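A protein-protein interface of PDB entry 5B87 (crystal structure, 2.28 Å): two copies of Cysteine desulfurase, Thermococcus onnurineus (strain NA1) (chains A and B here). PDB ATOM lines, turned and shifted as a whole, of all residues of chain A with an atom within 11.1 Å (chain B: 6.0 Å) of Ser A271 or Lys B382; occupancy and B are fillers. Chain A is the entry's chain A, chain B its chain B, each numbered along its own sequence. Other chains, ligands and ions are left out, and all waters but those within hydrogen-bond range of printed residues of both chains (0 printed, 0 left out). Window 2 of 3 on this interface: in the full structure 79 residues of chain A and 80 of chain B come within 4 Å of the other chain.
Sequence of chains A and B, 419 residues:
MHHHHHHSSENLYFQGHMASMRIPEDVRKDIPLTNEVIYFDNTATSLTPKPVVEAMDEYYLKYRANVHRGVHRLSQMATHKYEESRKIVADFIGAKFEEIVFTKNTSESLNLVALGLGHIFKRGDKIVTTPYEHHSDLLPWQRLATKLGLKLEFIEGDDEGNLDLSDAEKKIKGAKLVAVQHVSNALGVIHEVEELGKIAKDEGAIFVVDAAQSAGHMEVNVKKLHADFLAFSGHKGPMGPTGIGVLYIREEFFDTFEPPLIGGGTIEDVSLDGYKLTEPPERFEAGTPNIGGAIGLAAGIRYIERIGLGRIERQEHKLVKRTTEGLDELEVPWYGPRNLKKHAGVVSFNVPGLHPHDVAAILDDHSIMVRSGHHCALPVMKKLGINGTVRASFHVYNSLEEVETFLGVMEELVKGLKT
The side-chain amino group (NZ) of Lys B382 is in salt-bridge range of the side-chain carboxylate (OD1) of Asp A269, at 3.3 Å.
The side-chain amino group (NZ) of Lys B382 sits at hydrogen-bond distance from the backbone carbonyl oxygen (O) of Val A270 (2.9 Å).
NE2 of Gln B142 sits close to N of Gly A274, at 3.4 Å.
O of Leu A272 is in hydrogen-bond range of NE2 of Gln B142 (3.3 Å).
O of Ser A271 lies within hydrogen-bond range of NE2 of Gln B142, 2.8 Å away.
The backbone carbonyl oxygen (O) of Asp A269 sits at hydrogen-bond distance from the backbone NH (N) of Lys A276, at 3.0 Å.
The side-chain hydroxyl (OG) of Ser A271 lies within hydrogen-bond range of the backbone NH (N) of Gly A274, at 3.5 Å.
Leu B138 touches Val A270 (CD2 to CG1, 3.9 Å).
Leu B378 touches Val A270.
Ser A271 touches Lys B382 (CB to NZ, 3.8 Å).
CB of Pro B379 touches CD2 of Leu A272 (3.4 Å).
N of Asp A273 touches NE2 of Gln B142, 3.9 Å away.
OE1 of Gln B142 touches CD2 of Tyr A275 (3.6 Å).
Of the printed residues of chain B, Asp A269 touches Lys B382.
Of the printed residues of chain B, Val A270 touches Leu B138, Leu B378 and Lys B382.
Of chain B, only Gln B142 (2.8 Å) and Lys B382 (3.8 Å) come within 4 Å of Ser A271.
Of the printed residues of chain B, Leu A272 touches Gln B142 (3.3 Å) and Pro B379 (3.4 Å).
Printed residues of chain B within 4 Å of Gly A274: Gln B142 (3.4 Å).
Of the printed residues of chain A, Gln B142 touches Ser A271 (2.8 Å), Leu A272 (3.3 Å), Asp A273 (3.9 Å), Gly A274 (3.4 Å) and Tyr A275 (3.6 Å).
Ala B377 touches none of the printed residues of chain A.
Of chain A, only Val A270 comes within 4 Å of Leu B378.
Val B380 touches none of the printed residues of chain A.
No residue of chain A comes within 4 Å of Met B381.
Lys B382 touches just these residues of chain A: Asp A269 (3.3 Å), Val A270 (2.9 Å) and Ser A271 (3.8 Å).
Gly B385 touches none of the printed residues of chain A.
Ile B386 touches none of the printed residues of chain A.
The nearest residue of chain A that does not touch Lys B382 is Leu A272 (5.7 Å).
The nearest printed residue of chain B that does not touch Gly A274 is Lys B382 (6.5 Å).
Of the 12 printed residues of chain B, 5 touch a printed residue of chain A.
Printed residues of chain B that touch a printed residue of chain A: Leu B138, Gln B142, Leu B378, Pro B379 and Lys B382.
Hydrophobic or aromatic side chains of chain B that line the printed part of chain A: Leu B138, Leu B378 and Pro B379.
Hydrophobic or aromatic side chains of chain A within 4 Å of the printed part of chain B: Val A270, Leu A272 and Tyr A275.
Among the printed residues, 11 pairs touch across the chains.
Among the printed residues, Asp or Glu carboxylates within 4 Å of a Lys or Arg side-chain nitrogen of the other chain: Asp A269 with Lys B382 (3.3 Å).
No position is printed for both chains.
Of the 11 pairs that touch across the chains among the printed residues, none has its exchanged pair printed and touching as well.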
ATOM      1  N   ILE A 267       0.277   7.986   7.431  1.00  0.00           N
ATOM      2  CA  ILE A 267      -0.024   6.687   6.873  1.00  0.00           C
ATOM      3  C   ILE A 267       1.045   5.603   6.772  1.00  0.00           C
ATOM      4  O   ILE A 267       2.222   5.834   6.930  1.00  0.00           O
ATOM      5  CB  ILE A 267      -0.599   6.884   5.470  1.00  0.00           C
ATOM      6  CG1 ILE A 267       0.315   7.749   4.627  1.00  0.00           C
ATOM      7  CG2 ILE A 267      -1.910   7.618   5.535  1.00  0.00           C
ATOM      8  CD1 ILE A 267       1.633   7.115   4.295  1.00  0.00           C
ATOM      9  N   GLU A 268       0.588   4.395   6.494  1.00  0.00           N
ATOM     10  CA  GLU A 268       1.466   3.274   6.301  1.00  0.00           C
ATOM     11  C   GLU A 268       1.394   3.034   4.821  1.00  0.00           C
ATOM     12  O   GLU A 268       2.400   2.871   4.178  1.00  0.00           O
ATOM     13  CB  GLU A 268       0.972   2.073   7.054  1.00  0.00           C
ATOM     14  CG  GLU A 268       0.902   2.317   8.528  1.00  0.00           C
ATOM     15  CD  GLU A 268       1.810   1.403   9.298  1.00  0.00           C
ATOM     16  OE1 GLU A 268       2.923   1.842   9.633  1.00  0.00           O
ATOM     17  OE2 GLU A 268       1.409   0.246   9.547  1.00  0.00           O
ATOM     18  N   ASP A 269       0.182   3.037   4.292  1.00  0.00           N
ATOM     19  CA  ASP A 269      -0.040   2.875   2.845  1.00  0.00           C
ATOM     20  C   ASP A 269      -1.220   3.718   2.343  1.00  0.00           C
ATOM     21  O   ASP A 269      -2.156   4.006   3.089  1.00  0.00           O
ATOM     22  CB  ASP A 269      -0.283   1.384   2.496  1.00  0.00           C
ATOM     23  CG  ASP A 269      -0.344   1.128   0.991  1.00  0.00           C
ATOM     24  OD1 ASP A 269       0.613   1.521   0.277  1.00  0.00           O
ATOM     25  OD2 ASP A 269      -1.371   0.568   0.527  1.00  0.00           O
ATOM     26  N   VAL A 270      -1.175   4.041   1.064  1.00  0.00           N
ATOM     27  CA  VAL A 270      -2.209   4.800   0.412  1.00  0.00           C
ATOM     28  C   VAL A 270      -2.341   4.377  -1.040  1.00  0.00           C
ATOM     29  O   VAL A 270      -1.367   4.114  -1.695  1.00  0.00           O
ATOM     30  CB  VAL A 270      -1.868   6.304   0.353  1.00  0.00           C
ATOM     31  CG1 VAL A 270      -2.976   7.093  -0.290  1.00  0.00           C
ATOM     32  CG2 VAL A 270      -1.552   6.869   1.714  1.00  0.00           C
ATOM     33  N   SER A 271      -3.558   4.307  -1.537  1.00  0.00           N
ATOM     34  CA  SER A 271      -3.806   4.061  -2.947  1.00  0.00           C
ATOM     35  C   SER A 271      -4.856   5.076  -3.346  1.00  0.00           C
ATOM     36  O   SER A 271      -5.361   5.817  -2.489  1.00  0.00           O
ATOM     37  CB  SER A 271      -4.285   2.624  -3.178  1.00  0.00           C
ATOM     38  OG  SER A 271      -5.507   2.380  -2.512  1.00  0.00           O
ATOM     39  N   LEU A 272      -5.234   5.092  -4.611  1.00  0.00           N
ATOM     40  CA  LEU A 272      -6.273   5.999  -5.089  1.00  0.00           C
ATOM     41  C   LEU A 272      -7.670   5.802  -4.462  1.00  0.00           C
ATOM     42  O   LEU A 272      -8.449   6.717  -4.454  1.00  0.00           O
ATOM     43  CB  LEU A 272      -6.339   6.053  -6.608  1.00  0.00           C
ATOM     44  CG  LEU A 272      -5.075   6.569  -7.289  1.00  0.00           C
ATOM     45  CD1 LEU A 272      -4.803   8.056  -7.090  1.00  0.00           C
ATOM     46  CD2 LEU A 272      -3.885   5.723  -6.888  1.00  0.00           C
ATOM     47  N   ASP A 273      -8.017   4.644  -3.933  1.00  0.00           N
ATOM     48  CA  ASP A 273      -9.339   4.624  -3.229  1.00  0.00           C
ATOM     49  C   ASP A 273      -9.325   4.127  -1.772  1.00  0.00           C
ATOM     50  O   ASP A 273     -10.385   3.781  -1.241  1.00  0.00           O
ATOM     51  CB  ASP A 273     -10.481   4.006  -4.096  1.00  0.00           C
ATOM     52  CG  ASP A 273     -10.521   2.468  -4.071  1.00  0.00           C
ATOM     53  OD1 ASP A 273      -9.457   1.829  -4.257  1.00  0.00           O
ATOM     54  OD2 ASP A 273     -11.633   1.901  -3.890  1.00  0.00           O
ATOM     55  N   GLY A 274      -8.152   4.170  -1.118  1.00  0.00           N
ATOM     56  CA  GLY A 274      -8.019   3.761   0.298  1.00  0.00           C
ATOM     57  C   GLY A 274      -6.721   4.117   1.036  1.00  0.00           C
ATOM     58  O   GLY A 274      -5.658   4.265   0.418  1.00  0.00           O
ATOM     59  N   TYR A 275      -6.821   4.163   2.356  1.00  0.00           N
ATOM     60  CA  TYR A 275      -5.688   4.440   3.195  1.00  0.00           C
ATOM     61  C   TYR A 275      -5.633   3.657   4.520  1.00  0.00           C
ATOM     62  O   TYR A 275      -6.634   3.392   5.157  1.00  0.00           O
ATOM     63  CB  TYR A 275      -5.583   5.966   3.444  1.00  0.00           C
ATOM     64  CG  TYR A 275      -6.604   6.534   4.396  1.00  0.00           C
ATOM     65  CD1 TYR A 275      -6.474   6.358   5.741  1.00  0.00           C
ATOM     66  CD2 TYR A 275      -7.695   7.227   3.944  1.00  0.00           C
ATOM     67  CE1 TYR A 275      -7.401   6.838   6.613  1.00  0.00           C
ATOM     68  CE2 TYR A 275      -8.634   7.720   4.816  1.00  0.00           C
ATOM     69  CZ  TYR A 275      -8.474   7.505   6.152  1.00  0.00           C
ATOM     70  OH  TYR A 275      -9.379   7.976   7.038  1.00  0.00           O
ATOM     71  N   LYS A 276      -4.429   3.281   4.912  1.00  0.00           N
ATOM     72  CA  LYS A 276      -4.150   2.675   6.225  1.00  0.00           C
ATOM     73  C   LYS A 276      -3.331   3.668   7.024  1.00  0.00           C
ATOM     74  O   LYS A 276      -2.275   4.085   6.541  1.00  0.00           O
ATOM     75  CB  LYS A 276      -3.340   1.359   6.131  1.00  0.00           C
ATOM     76  CG  LYS A 276      -3.806   0.327   5.100  1.00  0.00           C
ATOM     77  CD  LYS A 276      -5.289  -0.051   5.198  1.00  0.00           C
ATOM     78  CE  LYS A 276      -5.603  -1.391   4.532  1.00  0.00           C
ATOM     79  NZ  LYS A 276      -4.924  -1.556   3.213  1.00  0.00           N
ATOM     80  N   LEU A 277      -3.793   4.012   8.244  1.00  0.00           N
ATOM     81  CA  LEU A 277      -3.066   4.955   9.160  1.00  0.00           C
ATOM     82  C   LEU A 277      -1.930   4.269   9.924  1.00  0.00           C
ATOM     83  O   LEU A 277      -1.991   3.066  10.162  1.00  0.00           O
ATOM     84  CB  LEU A 277      -4.000   5.600  10.200  1.00  0.00           C
ATOM     85  CG  LEU A 277      -5.218   6.412   9.751  1.00  0.00           C
ATOM     86  CD1 LEU A 277      -6.135   6.679  10.946  1.00  0.00           C
ATOM     87  CD2 LEU A 277      -4.782   7.701   9.087  1.00  0.00           C
ATOM     88  N   LEU B 138      -5.474  14.375  -0.670  1.00  0.00           N
ATOM     89  CA  LEU B 138      -6.086  13.118  -1.108  1.00  0.00           C
ATOM     90  C   LEU B 138      -6.890  12.513   0.053  1.00  0.00           C
ATOM     91  O   LEU B 138      -8.100  12.469  -0.030  1.00  0.00           O
ATOM     92  CB  LEU B 138      -5.004  12.136  -1.577  1.00  0.00           C
ATOM     93  CG  LEU B 138      -5.528  10.770  -2.086  1.00  0.00           C
ATOM     94  CD1 LEU B 138      -6.604  10.958  -3.148  1.00  0.00           C
ATOM     95  CD2 LEU B 138      -4.397   9.923  -2.637  1.00  0.00           C
ATOM     96  N   GLN B 142     -10.748  11.400   0.376  1.00  0.00           N
ATOM     97  CA  GLN B 142     -11.083   9.980   0.580  1.00  0.00           C
ATOM     98  C   GLN B 142     -11.980   9.768   1.796  1.00  0.00           C
ATOM     99  O   GLN B 142     -13.072   9.208   1.661  1.00  0.00           O
ATOM    100  CB  GLN B 142      -9.836   9.115   0.732  1.00  0.00           C
ATOM    101  CG  GLN B 142      -9.073   8.973  -0.562  1.00  0.00           C
ATOM    102  CD  GLN B 142      -7.752   8.256  -0.392  1.00  0.00           C
ATOM    103  OE1 GLN B 142      -7.050   8.430   0.601  1.00  0.00           O
ATOM    104  NE2 GLN B 142      -7.389   7.469  -1.387  1.00  0.00           N
ATOM    105  N   ALA B 377       3.617  10.661  -1.683  1.00  0.00           N
ATOM    106  CA  ALA B 377       2.863  10.661  -2.916  1.00  0.00           C
ATOM    107  C   ALA B 377       2.804   9.266  -3.538  1.00  0.00           C
ATOM    108  O   ALA B 377       2.965   9.104  -4.707  1.00  0.00           O
ATOM    109  CB  ALA B 377       3.426  11.673  -3.885  1.00  0.00           C
ATOM    110  N   LEU B 378       2.581   8.265  -2.708  1.00  0.00           N
ATOM    111  CA  LEU B 378       2.405   6.841  -3.131  1.00  0.00           C
ATOM    112  C   LEU B 378       1.572   6.534  -4.414  1.00  0.00           C
ATOM    113  O   LEU B 378       1.987   5.677  -5.195  1.00  0.00           O
ATOM    114  CB  LEU B 378       1.913   5.958  -1.946  1.00  0.00           C
ATOM    115  CG  LEU B 378       3.050   5.368  -1.121  1.00  0.00           C
ATOM    116  CD1 LEU B 378       2.654   5.148   0.337  1.00  0.00           C
ATOM    117  CD2 LEU B 378       3.533   4.081  -1.782  1.00  0.00           C
ATOM    118  N   PRO B 379       0.430   7.228  -4.652  1.00  0.00           N
ATOM    119  CA  PRO B 379      -0.249   7.002  -5.967  1.00  0.00           C
ATOM    120  C   PRO B 379       0.603   7.344  -7.234  1.00  0.00           C
ATOM    121  O   PRO B 379       0.426   6.707  -8.309  1.00  0.00           O
ATOM    122  CB  PRO B 379      -1.514   7.893  -5.875  1.00  0.00           C
ATOM    123  CG  PRO B 379      -1.221   8.901  -4.789  1.00  0.00           C
ATOM    124  CD  PRO B 379      -0.354   8.153  -3.797  1.00  0.00           C
ATOM    125  N   VAL B 380       1.509   8.323  -7.091  1.00  0.00           N
ATOM    126  CA  VAL B 380       2.480   8.655  -8.149  1.00  0.00           C
ATOM    127  C   VAL B 380       3.421   7.479  -8.386  1.00  0.00           C
ATOM    128  O   VAL B 380       3.687   7.157  -9.539  1.00  0.00           O
ATOM    129  CB  VAL B 380       3.329   9.910  -7.833  1.00  0.00           C
ATOM    130  CG1 VAL B 380       4.540  10.046  -8.772  1.00  0.00           C
ATOM    131  CG2 VAL B 380       2.464  11.152  -7.817  1.00  0.00           C
ATOM    132  N   MET B 381       3.953   6.896  -7.308  1.00  0.00           N
ATOM    133  CA  MET B 381       4.921   5.789  -7.419  1.00  0.00           C
ATOM    134  C   MET B 381       4.294   4.494  -8.018  1.00  0.00           C
ATOM    135  O   MET B 381       4.958   3.784  -8.786  1.00  0.00           O
ATOM    136  CB  MET B 381       5.609   5.498  -6.058  1.00  0.00           C
ATOM    137  CG  MET B 381       6.466   6.616  -5.468  1.00  0.00           C
ATOM    138  SD  MET B 381       7.521   7.492  -6.658  1.00  0.00           S
ATOM    139  CE  MET B 381       7.806   9.084  -5.859  1.00  0.00           C
ATOM    140  N   LYS B 382       3.049   4.201  -7.655  1.00  0.00           N
ATOM    141  CA  LYS B 382       2.307   3.017  -8.149  1.00  0.00           C
ATOM    142  C   LYS B 382       1.858   3.179  -9.613  1.00  0.00           C
ATOM    143  O   LYS B 382       2.003   2.241 -10.419  1.00  0.00           O
ATOM    144  CB  LYS B 382       1.066   2.736  -7.257  1.00  0.00           C
ATOM    145  CG  LYS B 382       1.403   2.289  -5.835  1.00  0.00           C
ATOM    146  CD  LYS B 382       0.176   2.297  -4.930  1.00  0.00           C
ATOM    147  CE  LYS B 382       0.505   1.782  -3.527  1.00  0.00           C
ATOM    148  NZ  LYS B 382      -0.711   1.450  -2.732  1.00  0.00           N
ATOM    149  N   LYS B 383       1.313   4.358  -9.938  1.00  0.00           N
ATOM    150  CA  LYS B 383       0.971   4.716 -11.315  1.00  0.00           C
ATOM    151  C   LYS B 383       2.151   4.445 -12.234  1.00  0.00           C
ATOM    152  O   LYS B 383       2.022   3.726 -13.213  1.00  0.00           O
ATOM    153  CB  LYS B 383       0.566   6.196 -11.434  1.00  0.00           C
ATOM    154  CG  LYS B 383       0.445   6.706 -12.874  1.00  0.00           C
ATOM    155  CD  LYS B 383      -0.197   8.082 -12.906  1.00  0.00           C
ATOM    156  CE  LYS B 383      -0.470   8.557 -14.321  1.00  0.00           C
ATOM    157  NZ  LYS B 383      -1.712   7.946 -14.868  1.00  0.00           N
ATOM    158  N   LEU B 384       3.292   5.034 -11.881  1.00  0.00           N
ATOM    159  CA  LEU B 384       4.563   4.853 -12.601  1.00  0.00           C
ATOM    160  C   LEU B 384       5.186   3.465 -12.487  1.00  0.00           C
ATOM    161  O   LEU B 384       5.963   3.104 -13.347  1.00  0.00           O
ATOM    162  CB  LEU B 384       5.588   5.896 -12.153  1.00  0.00           C
ATOM    163  CG  LEU B 384       5.517   7.188 -12.948  1.00  0.00           C
ATOM    164  CD1 LEU B 384       4.125   7.815 -12.914  1.00  0.00           C
ATOM    165  CD2 LEU B 384       6.591   8.137 -12.414  1.00  0.00           C
ATOM    166  N   GLY B 385       4.875   2.716 -11.429  1.00  0.00           N
ATOM    167  CA  GLY B 385       5.398   1.348 -11.244  1.00  0.00           C
ATOM    168  C   GLY B 385       6.851   1.294 -10.783  1.00  0.00           C
ATOM    169  O   GLY B 385       7.682   0.546 -11.338  1.00  0.00           O
ATOM    170  N   ILE B 386       7.151   2.087  -9.751  1.00  0.00           N
ATOM    171  CA  ILE B 386       8.482   2.132  -9.103  1.00  0.00           C
ATOM    172  C   ILE B 386       8.268   2.176  -7.584  1.00  0.00           C
ATOM    173  O   ILE B 386       7.149   2.448  -7.151  1.00  0.00           O
ATOM    174  CB  ILE B 386       9.308   3.329  -9.660  1.00  0.00           C
ATOM    175  CG1 ILE B 386       8.645   4.692  -9.298  1.00  0.00           C
ATOM    176  CG2 ILE B 386       9.497   3.173 -11.179  1.00  0.00           C
ATOM    177  CD1 ILE B 386       9.135   5.887 -10.085  1.00  0.00           C
